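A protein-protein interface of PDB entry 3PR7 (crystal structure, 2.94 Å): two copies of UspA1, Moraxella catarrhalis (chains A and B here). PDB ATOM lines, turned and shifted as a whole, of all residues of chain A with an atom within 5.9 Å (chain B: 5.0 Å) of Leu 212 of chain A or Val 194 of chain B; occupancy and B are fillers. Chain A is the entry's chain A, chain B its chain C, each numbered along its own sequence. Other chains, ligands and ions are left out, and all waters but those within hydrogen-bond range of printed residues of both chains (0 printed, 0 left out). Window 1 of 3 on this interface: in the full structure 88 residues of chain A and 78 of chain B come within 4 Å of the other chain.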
ATOM      1  N   VAL A 194     -31.011  37.906  19.017  1.00  0.00           N
ATOM      2  CA  VAL A 194     -30.321  37.308  17.883  1.00  0.00           C
ATOM      3  C   VAL A 194     -30.489  35.796  17.937  1.00  0.00           C
ATOM      4  O   VAL A 194     -30.331  35.184  19.002  1.00  0.00           O
ATOM      5  CB  VAL A 194     -28.807  37.658  17.891  1.00  0.00           C
ATOM      6  CG1 VAL A 194     -28.077  36.942  16.766  1.00  0.00           C
ATOM      7  CG2 VAL A 194     -28.592  39.161  17.789  1.00  0.00           C
ATOM      8  N   ALA A 195     -30.823  35.204  16.790  1.00  0.00           N
ATOM      9  CA  ALA A 195     -30.853  33.750  16.642  1.00  0.00           C
ATOM     10  C   ALA A 195     -30.139  33.338  15.363  1.00  0.00           C
ATOM     11  O   ALA A 195     -30.571  33.673  14.257  1.00  0.00           O
ATOM     12  CB  ALA A 195     -32.277  33.229  16.651  1.00  0.00           C
ATOM     13  N   ILE A 196     -29.028  32.626  15.529  1.00  0.00           N
ATOM     14  CA  ILE A 196     -28.263  32.105  14.403  1.00  0.00           C
ATOM     15  C   ILE A 196     -28.203  30.582  14.512  1.00  0.00           C
ATOM     16  O   ILE A 196     -27.764  30.039  15.534  1.00  0.00           O
ATOM     17  CB  ILE A 196     -26.844  32.718  14.343  1.00  0.00           C
ATOM     18  CG1 ILE A 196     -26.936  34.236  14.145  1.00  0.00           C
ATOM     19  CG2 ILE A 196     -26.032  32.080  13.219  1.00  0.00           C
ATOM     20  CD1 ILE A 196     -25.671  34.999  14.497  1.00  0.00           C
ATOM     21  N   GLY A 197     -28.662  29.909  13.460  1.00  0.00           N
ATOM     22  CA  GLY A 197     -28.712  28.456  13.423  1.00  0.00           C
ATOM     23  C   GLY A 197     -30.034  27.958  12.875  1.00  0.00           C
ATOM     24  O   GLY A 197     -30.501  28.430  11.838  1.00  0.00           O
ATOM     25  N   PHE A 210     -29.620  35.848  23.121  1.00  0.00           N
ATOM     26  CA  PHE A 210     -28.709  35.519  22.036  1.00  0.00           C
ATOM     27  C   PHE A 210     -28.572  34.013  21.885  1.00  0.00           C
ATOM     28  O   PHE A 210     -28.241  33.305  22.837  1.00  0.00           O
ATOM     29  CB  PHE A 210     -27.357  36.194  22.263  1.00  0.00           C
ATOM     30  CG  PHE A 210     -27.451  37.688  22.351  1.00  0.00           C
ATOM     31  CD1 PHE A 210     -27.332  38.474  21.209  1.00  0.00           C
ATOM     32  CD2 PHE A 210     -27.688  38.315  23.569  1.00  0.00           C
ATOM     33  CE1 PHE A 210     -27.437  39.858  21.283  1.00  0.00           C
ATOM     34  CE2 PHE A 210     -27.792  39.697  23.651  1.00  0.00           C
ATOM     35  CZ  PHE A 210     -27.670  40.467  22.506  1.00  0.00           C
ATOM     36  N   ILE A 211     -28.865  33.528  20.682  1.00  0.00           N
ATOM     37  CA  ILE A 211     -28.790  32.106  20.390  1.00  0.00           C
ATOM     38  C   ILE A 211     -27.861  31.846  19.216  1.00  0.00           C
ATOM     39  O   ILE A 211     -28.111  32.296  18.096  1.00  0.00           O
ATOM     40  CB  ILE A 211     -30.180  31.500  20.077  1.00  0.00           C
ATOM     41  CG1 ILE A 211     -31.141  31.704  21.253  1.00  0.00           C
ATOM     42  CG2 ILE A 211     -30.054  30.016  19.739  1.00  0.00           C
ATOM     43  CD1 ILE A 211     -32.606  31.487  20.904  1.00  0.00           C
ATOM     44  N   LEU A 212     -26.777  31.132  19.494  1.00  0.00           N
ATOM     45  CA  LEU A 212     -25.967  30.523  18.459  1.00  0.00           C
ATOM     46  C   LEU A 212     -26.112  29.024  18.673  1.00  0.00           C
ATOM     47  O   LEU A 212     -25.394  28.422  19.476  1.00  0.00           O
ATOM     48  CB  LEU A 212     -24.509  30.965  18.575  1.00  0.00           C
ATOM     49  CG  LEU A 212     -23.503  30.414  17.557  1.00  0.00           C
ATOM     50  CD1 LEU A 212     -23.826  30.860  16.132  1.00  0.00           C
ATOM     51  CD2 LEU A 212     -22.095  30.834  17.945  1.00  0.00           C
ATOM     52  N   GLY A 213     -27.076  28.432  17.980  1.00  0.00           N
ATOM     53  CA  GLY A 213     -27.391  27.028  18.174  1.00  0.00           C
ATOM     54  C   GLY A 213     -28.555  26.583  17.321  1.00  0.00           C
ATOM     55  O   GLY A 213     -29.000  27.306  16.430  1.00  0.00           O
ATOM     56  N   SER A 214     -29.040  25.377  17.596  1.00  0.00           N
ATOM     57  CA  SER A 214     -30.148  24.799  16.853  1.00  0.00           C
ATOM     58  C   SER A 214     -31.016  23.942  17.767  1.00  0.00           C
ATOM     59  O   SER A 214     -30.524  23.371  18.742  1.00  0.00           O
ATOM     60  CB  SER A 214     -29.640  23.984  15.657  1.00  0.00           C
ATOM     61  OG  SER A 214     -28.716  22.985  16.059  1.00  0.00           O
ATOM     62  N   LEU A 227     -27.865  31.221  24.685  1.00  0.00           N
ATOM     63  CA  LEU A 227     -27.964  29.790  24.429  1.00  0.00           C
ATOM     64  C   LEU A 227     -26.988  29.366  23.337  1.00  0.00           C
ATOM     65  O   LEU A 227     -27.016  29.891  22.217  1.00  0.00           O
ATOM     66  CB  LEU A 227     -29.398  29.402  24.052  1.00  0.00           C
ATOM     67  CG  LEU A 227     -30.437  29.242  25.170  1.00  0.00           C
ATOM     68  CD1 LEU A 227     -30.891  30.574  25.738  1.00  0.00           C
ATOM     69  CD2 LEU A 227     -31.634  28.474  24.655  1.00  0.00           C
ATOM     70  N   LEU A 228     -26.120  28.417  23.672  1.00  0.00           N
ATOM     71  CA  LEU A 228     -25.125  27.920  22.733  1.00  0.00           C
ATOM     72  C   LEU A 228     -25.307  26.438  22.441  1.00  0.00           C
ATOM     73  O   LEU A 228     -25.320  25.619  23.360  1.00  0.00           O
ATOM     74  CB  LEU A 228     -23.716  28.144  23.281  1.00  0.00           C
ATOM     75  CG  LEU A 228     -23.250  29.549  23.644  1.00  0.00           C
ATOM     76  CD1 LEU A 228     -21.886  29.460  24.314  1.00  0.00           C
ATOM     77  CD2 LEU A 228     -23.200  30.461  22.420  1.00  0.00           C
ATOM     78  N   GLY A 229     -25.452  26.097  21.164  1.00  0.00           N
ATOM     79  CA  GLY A 229     -25.394  24.702  20.740  1.00  0.00           C
ATOM     80  C   GLY A 229     -26.687  24.043  20.313  1.00  0.00           C
ATOM     81  O   GLY A 229     -27.777  24.593  20.463  1.00  0.00           O
ATOM     82  N   HIS A 230     -26.541  22.843  19.767  1.00  0.00           N
ATOM     83  CA  HIS A 230     -27.661  22.022  19.347  1.00  0.00           C
ATOM     84  C   HIS A 230     -28.336  21.442  20.583  1.00  0.00           C
ATOM     85  O   HIS A 230     -27.657  20.953  21.486  1.00  0.00           O
ATOM     86  CB  HIS A 230     -27.144  20.918  18.423  1.00  0.00           C
ATOM     87  CG  HIS A 230     -28.196  19.969  17.944  1.00  0.00           C
ATOM     88  ND1 HIS A 230     -29.306  20.377  17.236  1.00  0.00           N
ATOM     89  CD2 HIS A 230     -28.288  18.622  18.043  1.00  0.00           C
ATOM     90  CE1 HIS A 230     -30.045  19.324  16.935  1.00  0.00           C
ATOM     91  NE2 HIS A 230     -29.449  18.247  17.414  1.00  0.00           N
ATOM     92  N   VAL B 180     -24.348  28.546   7.397  1.00  0.00           N
ATOM     93  CA  VAL B 180     -24.068  29.975   7.504  1.00  0.00           C
ATOM     94  C   VAL B 180     -22.556  30.195   7.595  1.00  0.00           C
ATOM     95  O   VAL B 180     -21.926  29.804   8.583  1.00  0.00           O
ATOM     96  CB  VAL B 180     -24.775  30.600   8.733  1.00  0.00           C
ATOM     97  CG1 VAL B 180     -24.404  32.070   8.876  1.00  0.00           C
ATOM     98  CG2 VAL B 180     -26.282  30.445   8.623  1.00  0.00           C
ATOM     99  N   ILE B 188     -17.977  25.243   5.264  1.00  0.00           N
ATOM    100  CA  ILE B 188     -18.981  24.404   5.908  1.00  0.00           C
ATOM    101  C   ILE B 188     -19.522  23.372   4.938  1.00  0.00           C
ATOM    102  O   ILE B 188     -20.107  23.710   3.906  1.00  0.00           O
ATOM    103  CB  ILE B 188     -20.133  25.232   6.499  1.00  0.00           C
ATOM    104  CG1 ILE B 188     -19.593  26.166   7.578  1.00  0.00           C
ATOM    105  CG2 ILE B 188     -21.205  24.323   7.097  1.00  0.00           C
ATOM    106  CD1 ILE B 188     -20.414  27.391   7.751  1.00  0.00           C
ATOM    107  N   ASN B 192     -26.458  21.682   8.992  1.00  0.00           N
ATOM    108  CA  ASN B 192     -26.898  22.611  10.049  1.00  0.00           C
ATOM    109  C   ASN B 192     -25.772  23.140  10.927  1.00  0.00           C
ATOM    110  O   ASN B 192     -25.814  23.017  12.152  1.00  0.00           O
ATOM    111  CB  ASN B 192     -27.994  21.993  10.917  1.00  0.00           C
ATOM    112  CG  ASN B 192     -29.207  21.602  10.121  1.00  0.00           C
ATOM    113  OD1 ASN B 192     -29.848  22.440   9.491  1.00  0.00           O
ATOM    114  ND2 ASN B 192     -29.534  20.318  10.142  1.00  0.00           N
ATOM    115  N   SER B 193     -24.769  23.729  10.287  1.00  0.00           N
ATOM    116  CA  SER B 193     -23.616  24.260  10.994  1.00  0.00           C
ATOM    117  C   SER B 193     -23.395  25.731  10.662  1.00  0.00           C
ATOM    118  O   SER B 193     -23.897  26.233   9.650  1.00  0.00           O
ATOM    119  CB  SER B 193     -22.375  23.430  10.678  1.00  0.00           C
ATOM    120  OG  SER B 193     -22.452  22.165  11.312  1.00  0.00           O
ATOM    121  N   VAL B 194     -22.655  26.418  11.531  1.00  0.00           N
ATOM    122  CA  VAL B 194     -22.425  27.850  11.404  1.00  0.00           C
ATOM    123  C   VAL B 194     -20.966  28.155  11.707  1.00  0.00           C
ATOM    124  O   VAL B 194     -20.422  27.673  12.708  1.00  0.00           O
ATOM    125  CB  VAL B 194     -23.316  28.659  12.378  1.00  0.00           C
ATOM    126  CG1 VAL B 194     -22.998  30.143  12.301  1.00  0.00           C
ATOM    127  CG2 VAL B 194     -24.794  28.423  12.093  1.00  0.00           C
ATOM    128  N   ALA B 195     -20.339  28.947  10.837  1.00  0.00           N
ATOM    129  CA  ALA B 195     -18.994  29.460  11.078  1.00  0.00           C
ATOM    130  C   ALA B 195     -18.957  30.955  10.812  1.00  0.00           C
ATOM    131  O   ALA B 195     -19.178  31.402   9.681  1.00  0.00           O
ATOM    132  CB  ALA B 195     -17.980  28.741  10.220  1.00  0.00           C
ATOM    133  N   ILE B 196     -18.701  31.724  11.868  1.00  0.00           N
ATOM    134  CA  ILE B 196     -18.579  33.172  11.763  1.00  0.00           C
ATOM    135  C   ILE B 196     -17.193  33.575  12.257  1.00  0.00           C
ATOM    136  O   ILE B 196     -16.809  33.245  13.385  1.00  0.00           O
ATOM    137  CB  ILE B 196     -19.687  33.895  12.561  1.00  0.00           C
ATOM    138  CG1 ILE B 196     -21.066  33.545  11.990  1.00  0.00           C
ATOM    139  CG2 ILE B 196     -19.476  35.406  12.533  1.00  0.00           C
ATOM    140  CD1 ILE B 196     -22.228  33.834  12.926  1.00  0.00           C
ATOM    141  N   VAL B 209     -22.444  21.977  14.294  1.00  0.00           N
ATOM    142  CA  VAL B 209     -21.262  22.594  14.877  1.00  0.00           C
ATOM    143  C   VAL B 209     -21.353  24.108  14.716  1.00  0.00           C
ATOM    144  O   VAL B 209     -21.666  24.609  13.636  1.00  0.00           O
ATOM    145  CB  VAL B 209     -19.961  22.031  14.233  1.00  0.00           C
ATOM    146  CG1 VAL B 209     -18.750  22.901  14.562  1.00  0.00           C
ATOM    147  CG2 VAL B 209     -19.732  20.582  14.674  1.00  0.00           C
ATOM    148  N   PHE B 210     -21.080  24.832  15.796  1.00  0.00           N
ATOM    149  CA  PHE B 210     -21.166  26.284  15.780  1.00  0.00           C
ATOM    150  C   PHE B 210     -19.835  26.922  16.143  1.00  0.00           C
ATOM    151  O   PHE B 210     -19.268  26.644  17.200  1.00  0.00           O
ATOM    152  CB  PHE B 210     -22.289  26.751  16.702  1.00  0.00           C
ATOM    153  CG  PHE B 210     -23.626  26.196  16.327  1.00  0.00           C
ATOM    154  CD1 PHE B 210     -24.452  26.879  15.443  1.00  0.00           C
ATOM    155  CD2 PHE B 210     -24.054  24.971  16.831  1.00  0.00           C
ATOM    156  CE1 PHE B 210     -25.690  26.359  15.077  1.00  0.00           C
ATOM    157  CE2 PHE B 210     -25.291  24.443  16.474  1.00  0.00           C
ATOM    158  CZ  PHE B 210     -26.107  25.135  15.594  1.00  0.00           C
ATOM    159  N   ILE B 211     -19.334  27.764  15.243  1.00  0.00           N
ATOM    160  CA  ILE B 211     -18.064  28.441  15.446  1.00  0.00           C
ATOM    161  C   ILE B 211     -18.244  29.947  15.358  1.00  0.00           C
ATOM    162  O   ILE B 211     -18.652  30.481  14.324  1.00  0.00           O
ATOM    163  CB  ILE B 211     -16.995  27.998  14.418  1.00  0.00           C
ATOM    164  CG1 ILE B 211     -16.780  26.481  14.474  1.00  0.00           C
ATOM    165  CG2 ILE B 211     -15.678  28.752  14.652  1.00  0.00           C
ATOM    166  CD1 ILE B 211     -16.032  25.913  13.274  1.00  0.00           C
ATOM    167  N   LEU B 212     -17.955  30.617  16.464  1.00  0.00           N
ATOM    168  CA  LEU B 212     -17.765  32.052  16.481  1.00  0.00           C
ATOM    169  C   LEU B 212     -16.313  32.236  16.900  1.00  0.00           C
ATOM    170  O   LEU B 212     -15.988  32.240  18.093  1.00  0.00           O
ATOM    171  CB  LEU B 212     -18.723  32.717  17.472  1.00  0.00           C
ATOM    172  CG  LEU B 212     -18.650  34.238  17.627  1.00  0.00           C
ATOM    173  CD1 LEU B 212     -19.009  34.965  16.330  1.00  0.00           C
ATOM    174  CD2 LEU B 212     -19.551  34.682  18.765  1.00  0.00           C
ATOM    175  N   LEU B 228     -15.477  28.713  20.412  1.00  0.00           N
ATOM    176  CA  LEU B 228     -15.448  30.154  20.594  1.00  0.00           C
ATOM    177  C   LEU B 228     -14.021  30.677  20.632  1.00  0.00           C
ATOM    178  O   LEU B 228     -13.209  30.208  21.434  1.00  0.00           O
ATOM    179  CB  LEU B 228     -16.154  30.543  21.895  1.00  0.00           C
ATOM    180  CG  LEU B 228     -17.617  30.158  22.120  1.00  0.00           C
ATOM    181  CD1 LEU B 228     -18.010  30.515  23.540  1.00  0.00           C
ATOM    182  CD2 LEU B 228     -18.550  30.831  21.109  1.00  0.00           C
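The side-chain hydroxyl of Ser 214 of chain A is in hydrogen-bond range of a ring nitrogen (ND1) of His 230 of chain A (2.9 Å). The backbone NH of Ser 214 of chain A sits at hydrogen-bond distance from the backbone carbonyl oxygen of Gly 229 of chain A (3.2 Å). O of Leu 227 of chain A lies within hydrogen-bond range of N of Leu 212 of chain A (3.0 Å). N of Ile 211 of chain B lies within hydrogen-bond range of O of Val 194 of chain B, 2.8 Å away. The backbone carbonyl oxygen of Ile 211 of chain B lies within hydrogen-bond range of the backbone NH of Ile 196 of chain B. The backbone carbonyl oxygen of Ile 196 of chain A sits at hydrogen-bond distance from the backbone NH of Gly 213 of chain A.
Printed residues of chain B within 4 Å of Ile 196 of chain A: Val 194 and Ile 196. Printed residues of chain B within 4 Å of Gly 213 of chain A: Phe 210 (3.3 Å). Printed residues of chain B within 4 Å of Ser 214 of chain A: Phe 210 (3.4 Å). Printed residues of chain A within 4 Å of Val 194 of chain B: Ile 196 and Leu 212. Printed residues of chain A within 4 Å of Ile 196 of chain B: Ile 196. Printed residues of chain A within 4 Å of Leu 212 of chain B: Leu 212.
CG1 of Val 194 of chain B touches CG2 of Ile 196 of chain A, at 3.7 Å. Ile 196 of chain A touches Ile 196 of chain B (CD1 to CD1, 3.96 Å). Val 194 of chain B touches Leu 212 of chain A (CG1 to CD1, 3.98 Å). Leu 212 of chain A touches Phe 210 of chain B (CG to CB, 3.95 Å). CB of Leu 212 of chain B touches CD2 of Leu 212 of chain A (3.9 Å). Phe 210 of chain B touches Gly 213 of chain A (CZ to C, 3.3 Å). Ser 214 of chain A touches Phe 210 of chain B (OG to CZ, 3.4 Å). N of His 230 of chain A touches CE2 of Phe 210 of chain B, 3.9 Å away.
Of the 12 printed residues of chain B, 4 touch a printed residue of chain A. Printed residues of chain B that touch a printed residue of chain A: Val 194, Ile 196, Phe 210 and Leu 212. Along chain B the printed residues that touch a printed residue of chain A span positions 194 to 212. Hydrophobic or aromatic side chains of chain A within 4 Å of the printed part of chain B: Ile 196 and Leu 212. Among the printed residues, 8 pairs touch across the chains. Among the printed residues, no Asp or Glu carboxylate lies within 4 Å of a Lys or Arg side-chain nitrogen of the other chain.
Ile 196 of chain A touches Val 194 of chain B, but with the chains exchanged Val 194 of chain A does not touch Ile 196 of chain B (7.7 Å). Ile 196 of chain B touches its own counterpart, Ile 196 of chain A. Leu 212 of chain A touches Val 194 of chain B, but with the chains exchanged Val 194 of chain A does not touch Leu 212 of chain B (9.0 Å). Leu 212 of chain A touches Phe 210 of chain B, but with the chains exchanged Phe 210 of chain A does not touch Leu 212 of chain B (8.7 Å). Positions printed for both chains: 194, 195, 196, 210, 211, 212 and 228. Of the 8 pairs that touch across the chains among the printed residues, 2 have their exchanged pair printed and touching as well.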
